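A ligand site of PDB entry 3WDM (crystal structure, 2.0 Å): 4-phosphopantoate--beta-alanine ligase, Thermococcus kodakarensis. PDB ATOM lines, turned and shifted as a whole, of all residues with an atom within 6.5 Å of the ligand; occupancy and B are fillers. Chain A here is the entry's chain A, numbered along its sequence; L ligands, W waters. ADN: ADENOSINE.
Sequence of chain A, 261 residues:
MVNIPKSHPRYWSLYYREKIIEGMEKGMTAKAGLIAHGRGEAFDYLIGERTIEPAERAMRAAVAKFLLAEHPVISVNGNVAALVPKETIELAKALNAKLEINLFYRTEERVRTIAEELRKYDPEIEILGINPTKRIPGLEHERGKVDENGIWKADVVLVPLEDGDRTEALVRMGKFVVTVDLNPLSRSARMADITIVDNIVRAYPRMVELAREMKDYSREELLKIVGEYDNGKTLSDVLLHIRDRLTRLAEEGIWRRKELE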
ATOM      1  N   ALA A  36      25.418  10.078   5.107  1.00  0.00           N
ATOM      2  CA  ALA A  36      24.489  11.166   5.435  1.00  0.00           C
ATOM      3  C   ALA A  36      24.147  11.155   6.932  1.00  0.00           C
ATOM      4  O   ALA A  36      23.991  12.212   7.540  1.00  0.00           O
ATOM      5  CB  ALA A  36      23.214  11.063   4.594  1.00  0.00           C
ATOM      6  N   HIS A  37      24.050   9.982   7.545  1.00  0.00           N
ATOM      7  CA  HIS A  37      23.720   9.910   8.975  1.00  0.00           C
ATOM      8  C   HIS A  37      24.846  10.616   9.752  1.00  0.00           C
ATOM      9  O   HIS A  37      24.583  11.367  10.707  1.00  0.00           O
ATOM     10  CB  HIS A  37      23.625   8.462   9.453  1.00  0.00           C
ATOM     11  CG  HIS A  37      23.175   8.330  10.875  1.00  0.00           C
ATOM     12  ND1 HIS A  37      21.872   8.591  11.273  1.00  0.00           N
ATOM     13  CD2 HIS A  37      23.848   8.014  12.011  1.00  0.00           C
ATOM     14  CE1 HIS A  37      21.778   8.452  12.588  1.00  0.00           C
ATOM     15  NE2 HIS A  37      22.963   8.107  13.058  1.00  0.00           N
ATOM     16  N   GLY A  38      26.086  10.380   9.328  1.00  0.00           N
ATOM     17  CA  GLY A  38      27.224  10.993   9.959  1.00  0.00           C
ATOM     18  C   GLY A  38      27.231  12.502   9.829  1.00  0.00           C
ATOM     19  O   GLY A  38      27.584  13.210  10.778  1.00  0.00           O
ATOM     20  N   ARG A  39      26.832  13.005   8.669  1.00  0.00           N
ATOM     21  CA  ARG A  39      26.778  14.449   8.464  1.00  0.00           C
ATOM     22  C   ARG A  39      25.774  15.062   9.442  1.00  0.00           C
ATOM     23  O   ARG A  39      26.000  16.153   9.988  1.00  0.00           O
ATOM     24  CB  ARG A  39      26.382  14.801   7.021  1.00  0.00           C
ATOM     25  CG  ARG A  39      27.462  14.471   5.979  1.00  0.00           C
ATOM     26  CD  ARG A  39      27.292  15.286   4.691  1.00  0.00           C
ATOM     27  NE  ARG A  39      26.070  14.966   3.950  1.00  0.00           N
ATOM     28  CZ  ARG A  39      25.900  13.902   3.174  1.00  0.00           C
ATOM     29  NH1 ARG A  39      26.886  13.028   3.036  1.00  0.00           N
ATOM     30  NH2 ARG A  39      24.738  13.701   2.563  1.00  0.00           N
ATOM     31  N   GLY A  40      24.663  14.361   9.666  1.00  0.00           N
ATOM     32  CA  GLY A  40      23.670  14.843  10.604  1.00  0.00           C
ATOM     33  C   GLY A  40      24.241  14.883  12.017  1.00  0.00           C
ATOM     34  O   GLY A  40      24.079  15.867  12.760  1.00  0.00           O
ATOM     35  N   GLU A  41      24.942  13.811  12.394  1.00  0.00           N
ATOM     36  CA  GLU A  41      25.530  13.726  13.726  1.00  0.00           C
ATOM     37  C   GLU A  41      26.473  14.885  14.027  1.00  0.00           C
ATOM     38  O   GLU A  41      26.485  15.383  15.153  1.00  0.00           O
ATOM     39  CB  GLU A  41      26.290  12.429  13.882  1.00  0.00           C
ATOM     40  CG  GLU A  41      25.454  11.171  13.842  1.00  0.00           C
ATOM     41  CD  GLU A  41      26.283   9.962  14.138  1.00  0.00           C
ATOM     42  OE1 GLU A  41      27.269   9.737  13.426  1.00  0.00           O
ATOM     43  OE2 GLU A  41      25.964   9.237  15.104  1.00  0.00           O
ATOM     44  N   PHE A  43      26.428  17.943  12.883  1.00  0.00           N
ATOM     45  CA  PHE A  43      25.660  19.125  13.221  1.00  0.00           C
ATOM     46  C   PHE A  43      25.000  18.930  14.590  1.00  0.00           C
ATOM     47  O   PHE A  43      24.861  19.885  15.337  1.00  0.00           O
ATOM     48  CB  PHE A  43      24.628  19.409  12.132  1.00  0.00           C
ATOM     49  CG  PHE A  43      25.222  20.123  10.938  1.00  0.00           C
ATOM     50  CD1 PHE A  43      25.464  21.502  10.976  1.00  0.00           C
ATOM     51  CD2 PHE A  43      25.592  19.413   9.794  1.00  0.00           C
ATOM     52  CE1 PHE A  43      26.069  22.151   9.892  1.00  0.00           C
ATOM     53  CE2 PHE A  43      26.193  20.055   8.727  1.00  0.00           C
ATOM     54  CZ  PHE A  43      26.433  21.431   8.774  1.00  0.00           C
ATOM     55  N   ASP A  44      24.628  17.704  14.939  1.00  0.00           N
ATOM     56  CA  ASP A  44      24.015  17.497  16.236  1.00  0.00           C
ATOM     57  C   ASP A  44      25.034  17.803  17.322  1.00  0.00           C
ATOM     58  O   ASP A  44      24.684  18.322  18.382  1.00  0.00           O
ATOM     59  CB  ASP A  44      23.474  16.070  16.396  1.00  0.00           C
ATOM     60  CG  ASP A  44      22.147  16.036  17.176  1.00  0.00           C
ATOM     61  OD1 ASP A  44      21.656  17.103  17.632  1.00  0.00           O
ATOM     62  OD2 ASP A  44      21.593  14.933  17.322  1.00  0.00           O
ATOM     63  N   ASN A  77      12.106   7.841   3.416  1.00  0.00           N
ATOM     64  CA  ASN A  77      13.260   7.339   2.663  1.00  0.00           C
ATOM     65  C   ASN A  77      13.971   6.271   3.487  1.00  0.00           C
ATOM     66  O   ASN A  77      13.485   5.894   4.557  1.00  0.00           O
ATOM     67  CB  ASN A  77      14.239   8.461   2.248  1.00  0.00           C
ATOM     68  CG  ASN A  77      14.766   9.252   3.417  1.00  0.00           C
ATOM     69  OD1 ASN A  77      15.093   8.706   4.465  1.00  0.00           O
ATOM     70  ND2 ASN A  77      14.873  10.573   3.233  1.00  0.00           N
ATOM     71  N   ASN A  79      16.773   6.282   5.303  1.00  0.00           N
ATOM     72  CA  ASN A  79      17.244   6.671   6.615  1.00  0.00           C
ATOM     73  C   ASN A  79      16.038   6.800   7.545  1.00  0.00           C
ATOM     74  O   ASN A  79      16.084   6.373   8.686  1.00  0.00           O
ATOM     75  CB  ASN A  79      18.003   8.012   6.537  1.00  0.00           C
ATOM     76  CG  ASN A  79      19.451   7.821   6.136  1.00  0.00           C
ATOM     77  OD1 ASN A  79      19.754   7.159   5.138  1.00  0.00           O
ATOM     78  ND2 ASN A  79      20.369   8.417   6.908  1.00  0.00           N
ATOM     79  N   LEU A  83      15.399   4.644  11.145  1.00  0.00           N
ATOM     80  CA  LEU A  83      15.395   5.311  12.447  1.00  0.00           C
ATOM     81  C   LEU A  83      14.090   5.558  13.170  1.00  0.00           C
ATOM     82  O   LEU A  83      14.056   5.482  14.393  1.00  0.00           O
ATOM     83  CB  LEU A  83      16.127   6.653  12.331  1.00  0.00           C
ATOM     84  CG  LEU A  83      17.528   6.574  11.710  1.00  0.00           C
ATOM     85  CD1 LEU A  83      18.008   7.967  11.289  1.00  0.00           C
ATOM     86  CD2 LEU A  83      18.474   5.949  12.728  1.00  0.00           C
ATOM     87  N   PRO A 160      11.791  14.849   5.183  1.00  0.00           N
ATOM     88  CA  PRO A 160      12.937  14.894   6.091  1.00  0.00           C
ATOM     89  C   PRO A 160      14.224  14.337   5.490  1.00  0.00           C
ATOM     90  O   PRO A 160      14.179  13.543   4.556  1.00  0.00           O
ATOM     91  CB  PRO A 160      12.434  14.094   7.281  1.00  0.00           C
ATOM     92  CG  PRO A 160      11.643  12.991   6.619  1.00  0.00           C
ATOM     93  CD  PRO A 160      10.875  13.735   5.527  1.00  0.00           C
ATOM     94  N   LEU A 161      15.366  14.746   6.050  1.00  0.00           N
ATOM     95  CA  LEU A 161      16.677  14.267   5.608  1.00  0.00           C
ATOM     96  C   LEU A 161      16.654  14.162   4.099  1.00  0.00           C
ATOM     97  O   LEU A 161      16.963  13.109   3.529  1.00  0.00           O
ATOM     98  CB  LEU A 161      16.960  12.889   6.238  1.00  0.00           C
ATOM     99  CG  LEU A 161      17.250  12.826   7.741  1.00  0.00           C
ATOM    100  CD1 LEU A 161      16.164  13.510   8.530  1.00  0.00           C
ATOM    101  CD2 LEU A 161      17.398  11.373   8.185  1.00  0.00           C
ATOM    102  N   GLU A 162      16.273  15.260   3.465  1.00  0.00           N
ATOM    103  CA  GLU A 162      16.094  15.303   2.024  1.00  0.00           C
ATOM    104  C   GLU A 162      17.091  16.094   1.223  1.00  0.00           C
ATOM    105  O   GLU A 162      17.717  17.051   1.698  1.00  0.00           O
ATOM    106  CB  GLU A 162      14.703  15.801   1.712  1.00  0.00           C
ATOM    107  N   ASP A 163      17.204  15.686  -0.036  1.00  0.00           N
ATOM    108  CA  ASP A 163      18.110  16.316  -0.980  1.00  0.00           C
ATOM    109  C   ASP A 163      17.590  17.715  -1.324  1.00  0.00           C
ATOM    110  O   ASP A 163      16.383  17.914  -1.516  1.00  0.00           O
ATOM    111  CB  ASP A 163      18.238  15.439  -2.229  1.00  0.00           C
ATOM    112  CG  ASP A 163      18.982  16.122  -3.355  1.00  0.00           C
ATOM    113  OD1 ASP A 163      18.387  17.000  -4.019  1.00  0.00           O
ATOM    114  OD2 ASP A 163      20.175  15.773  -3.560  1.00  0.00           O
ATOM    115  N   VAL A 180      12.955  18.359   8.018  1.00  0.00           N
ATOM    116  CA  VAL A 180      13.677  18.160   9.268  1.00  0.00           C
ATOM    117  C   VAL A 180      15.105  17.928   8.768  1.00  0.00           C
ATOM    118  O   VAL A 180      15.370  17.002   7.996  1.00  0.00           O
ATOM    119  CB  VAL A 180      13.162  16.906  10.037  1.00  0.00           C
ATOM    120  CG1 VAL A 180      14.080  16.603  11.246  1.00  0.00           C
ATOM    121  CG2 VAL A 180      11.742  17.157  10.513  1.00  0.00           C
ATOM    122  N   ASP A 181      16.035  18.788   9.186  1.00  0.00           N
ATOM    123  CA  ASP A 181      17.434  18.692   8.724  1.00  0.00           C
ATOM    124  C   ASP A 181      18.311  19.344   9.785  1.00  0.00           C
ATOM    125  O   ASP A 181      18.101  20.509  10.137  1.00  0.00           O
ATOM    126  CB  ASP A 181      17.598  19.458   7.406  1.00  0.00           C
ATOM    127  CG  ASP A 181      18.840  19.026   6.603  1.00  0.00           C
ATOM    128  OD1 ASP A 181      19.886  18.740   7.230  1.00  0.00           O
ATOM    129  OD2 ASP A 181      18.751  18.986   5.349  1.00  0.00           O
ATOM    130  N   LEU A 182      19.282  18.581  10.287  1.00  0.00           N
ATOM    131  CA  LEU A 182      20.185  19.080  11.303  1.00  0.00           C
ATOM    132  C   LEU A 182      21.154  20.154  10.778  1.00  0.00           C
ATOM    133  O   LEU A 182      21.752  20.884  11.562  1.00  0.00           O
ATOM    134  CB  LEU A 182      20.952  17.906  11.942  1.00  0.00           C
ATOM    135  CG  LEU A 182      20.281  17.271  13.171  1.00  0.00           C
ATOM    136  CD1 LEU A 182      20.812  15.875  13.431  1.00  0.00           C
ATOM    137  CD2 LEU A 182      20.512  18.148  14.394  1.00  0.00           C
ATOM    138  N   ASN A 183      21.307  20.239   9.454  1.00  0.00           N
ATOM    139  CA  ASN A 183      22.174  21.250   8.846  1.00  0.00           C
ATOM    140  C   ASN A 183      21.346  22.465   8.464  1.00  0.00           C
ATOM    141  O   ASN A 183      20.647  22.449   7.474  1.00  0.00           O
ATOM    142  CB  ASN A 183      22.883  20.702   7.604  1.00  0.00           C
ATOM    143  CG  ASN A 183      23.784  21.739   6.948  1.00  0.00           C
ATOM    144  OD1 ASN A 183      23.961  22.829   7.471  1.00  0.00           O
ATOM    145  ND2 ASN A 183      24.386  21.379   5.813  1.00  0.00           N
ATOM    146  N   PRO A 184      21.435  23.538   9.236  1.00  0.00           N
ATOM    147  CA  PRO A 184      20.680  24.764   8.965  1.00  0.00           C
ATOM    148  C   PRO A 184      21.114  25.506   7.690  1.00  0.00           C
ATOM    149  O   PRO A 184      20.408  26.414   7.233  1.00  0.00           O
ATOM    150  CB  PRO A 184      20.943  25.614  10.206  1.00  0.00           C
ATOM    151  CG  PRO A 184      22.342  25.210  10.580  1.00  0.00           C
ATOM    152  CD  PRO A 184      22.296  23.697  10.423  1.00  0.00           C
ATOM    153  N   SER A 186      22.006  23.762   4.793  1.00  0.00           N
ATOM    154  CA  SER A 186      21.841  22.946   3.600  1.00  0.00           C
ATOM    155  C   SER A 186      20.848  23.619   2.646  1.00  0.00           C
ATOM    156  O   SER A 186      20.060  24.471   3.076  1.00  0.00           O
ATOM    157  CB  SER A 186      21.365  21.550   3.976  1.00  0.00           C
ATOM    158  OG  SER A 186      20.022  21.569   4.408  1.00  0.00           O
ATOM    159  N   ILE A 196      12.834  22.356  10.319  1.00  0.00           N
ATOM    160  CA  ILE A 196      12.955  21.885  11.691  1.00  0.00           C
ATOM    161  C   ILE A 196      14.394  21.392  11.873  1.00  0.00           C
ATOM    162  O   ILE A 196      14.760  20.318  11.396  1.00  0.00           O
ATOM    163  CB  ILE A 196      11.979  20.683  11.985  1.00  0.00           C
ATOM    164  CG1 ILE A 196      10.526  21.167  11.975  1.00  0.00           C
ATOM    165  CG2 ILE A 196      12.321  20.060  13.337  1.00  0.00           C
ATOM    166  CD1 ILE A 196       9.532  20.108  11.460  1.00  0.00           C
ATOM    167  N   ASP A 198      16.573  19.739  13.986  1.00  0.00           N
ATOM    168  CA  ASP A 198      16.626  18.897  15.147  1.00  0.00           C
ATOM    169  C   ASP A 198      16.831  17.501  14.566  1.00  0.00           C
ATOM    170  O   ASP A 198      16.624  17.283  13.365  1.00  0.00           O
ATOM    171  CB  ASP A 198      15.283  19.010  15.884  1.00  0.00           C
ATOM    172  CG  ASP A 198      15.290  18.372  17.283  1.00  0.00           C
ATOM    173  OD1 ASP A 198      16.376  18.028  17.796  1.00  0.00           O
ATOM    174  OD2 ASP A 198      14.187  18.231  17.872  1.00  0.00           O
ATOM    175  N   ASN A 199      17.276  16.575  15.408  1.00  0.00           N
ATOM    176  CA  ASN A 199      17.495  15.213  14.966  1.00  0.00           C
ATOM    177  C   ASN A 199      16.117  14.572  14.776  1.00  0.00           C
ATOM    178  O   ASN A 199      15.244  14.702  15.641  1.00  0.00           O
ATOM    179  CB  ASN A 199      18.281  14.445  16.031  1.00  0.00           C
ATOM    180  CG  ASN A 199      18.827  13.142  15.524  1.00  0.00           C
ATOM    181  OD1 ASN A 199      18.087  12.329  14.938  1.00  0.00           O
ATOM    182  ND2 ASN A 199      20.127  12.913  15.737  1.00  0.00           N
ATOM    183  N   ILE A 200      15.929  13.859  13.664  1.00  0.00           N
ATOM    184  CA  ILE A 200      14.630  13.255  13.430  1.00  0.00           C
ATOM    185  C   ILE A 200      14.187  12.310  14.564  1.00  0.00           C
ATOM    186  O   ILE A 200      12.982  12.133  14.794  1.00  0.00           O
ATOM    187  CB  ILE A 200      14.561  12.521  12.061  1.00  0.00           C
ATOM    188  CG1 ILE A 200      13.096  12.216  11.723  1.00  0.00           C
ATOM    189  CG2 ILE A 200      15.406  11.241  12.066  1.00  0.00           C
ATOM    190  CD1 ILE A 200      12.873  11.798  10.281  1.00  0.00           C
ATOM    191  N   VAL A 201      15.143  11.746  15.299  1.00  0.00           N
ATOM    192  CA  VAL A 201      14.758  10.840  16.396  1.00  0.00           C
ATOM    193  C   VAL A 201      14.139  11.611  17.574  1.00  0.00           C
ATOM    194  O   VAL A 201      13.468  11.032  18.417  1.00  0.00           O
ATOM    195  CB  VAL A 201      15.951   9.968  16.883  1.00  0.00           C
ATOM    196  CG1 VAL A 201      16.434   9.106  15.746  1.00  0.00           C
ATOM    197  CG2 VAL A 201      17.083  10.853  17.415  1.00  0.00           C
HETATM  198  O5' ADN L   1      20.321  13.993   3.633  1.00  0.00           O
HETATM  199  C5' ADN L   1      21.428  14.615   4.283  1.00  0.00           C
HETATM  200  C4' ADN L   1      20.938  15.692   5.274  1.00  0.00           C
HETATM  201  O4' ADN L   1      20.112  15.085   6.301  1.00  0.00           O
HETATM  202  C3' ADN L   1      22.144  16.344   5.959  1.00  0.00           C
HETATM  203  O3' ADN L   1      22.250  17.718   5.564  1.00  0.00           O
HETATM  204  C2' ADN L   1      21.901  16.246   7.477  1.00  0.00           C
HETATM  205  O2' ADN L   1      21.896  17.543   8.076  1.00  0.00           O
HETATM  206  C1' ADN L   1      20.523  15.588   7.590  1.00  0.00           C
HETATM  207  N9  ADN L   1      20.480  14.516   8.589  1.00  0.00           N
HETATM  208  C8  ADN L   1      21.230  13.367   8.648  1.00  0.00           C
HETATM  209  N7  ADN L   1      20.864  12.653   9.684  1.00  0.00           N
HETATM  210  C5  ADN L   1      19.858  13.306  10.335  1.00  0.00           C
HETATM  211  C6  ADN L   1      19.061  13.048  11.490  1.00  0.00           C
HETATM  212  N6  ADN L   1      19.249  11.896  12.212  1.00  0.00           N
HETATM  213  N1  ADN L   1      18.122  13.964  11.856  1.00  0.00           N
HETATM  214  C2  ADN L   1      17.927  15.104  11.161  1.00  0.00           C
HETATM  215  N3  ADN L   1      18.651  15.385  10.064  1.00  0.00           N
HETATM  216  C4  ADN L   1      19.611  14.517   9.635  1.00  0.00           C
HETATM  217  O   HOH W   1      19.961  18.035   2.941  1.00  0.00           O
HETATM  218  O   HOH W   2      20.213   9.699   9.312  1.00  0.00           O
HETATM  219  O   HOH W   3      22.227  11.674  12.480  1.00  0.00           O
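OD1 of Asp 181 is in hydrogen-bond range of O2' of the ligand (2.5 Å). N of Ile 200 is in hydrogen-bond range of N1 of the ligand (2.8 Å). The side-chain amide oxygen of Asn 199 sits at hydrogen-bond distance from a nitrogen (N6) of the ligand, at 3.0 Å. O2' of the ligand sits at hydrogen-bond distance from N of Asn 183, at 3.1 Å. The backbone NH of Leu 182 sits at hydrogen-bond distance from a nitrogen (N3) of the ligand, at 3.3 Å. The backbone carbonyl oxygen (O) of Leu 161 lies within hydrogen-bond range of an oxygen (O5') of the ligand.
OD1 of Asp 181 sits at hydrogen-bond distance from N of Asn 183. OD2 of Asp 181 is in hydrogen-bond range of OG of Ser 186 (3.0 Å). The backbone carbonyl oxygen (O) of Ile 196 is in hydrogen-bond range of the backbone NH (N) of Asp 181. N of Val 201 is in hydrogen-bond range of OD1 of Asn 199, 3.0 Å away. OD2 of Asp 44 lies within hydrogen-bond range of ND2 of Asn 199, at 3.0 Å. O of Asn 183 sits at hydrogen-bond distance from OG of Ser 186, at 3.3 Å. The backbone carbonyl oxygen of Val 180 sits at hydrogen-bond distance from the backbone NH of Leu 161 (3.0 Å). ND2 of Asn 77 lies within hydrogen-bond range of O of Leu 161.
Merely in contact with the ligand: Ala 36, Arg 39, Gly 40 and Asp 198. The nearest printed residue that does not touch the ligand is His 37 (4.02 Å).
Water W3 lies within hydrogen-bond range of the backbone carbonyl oxygen of His 37 (3.0 Å), a nitrogen (N6) of the ligand (3.0 Å) and the backbone NH of Glu 41 (3.5 Å). Water W2 lies within hydrogen-bond range of ND2 of Asn 79 (2.7 Å), ND1 of His 37 (2.8 Å) and N7 of the ligand (3.0 Å). Water W1 lies within hydrogen-bond range of the backbone carbonyl oxygen (O) of Glu 162 (2.7 Å), the side-chain carboxylate (OD2) of Asp 181 (2.9 Å) and an oxygen (O3') of the ligand (3.5 Å).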
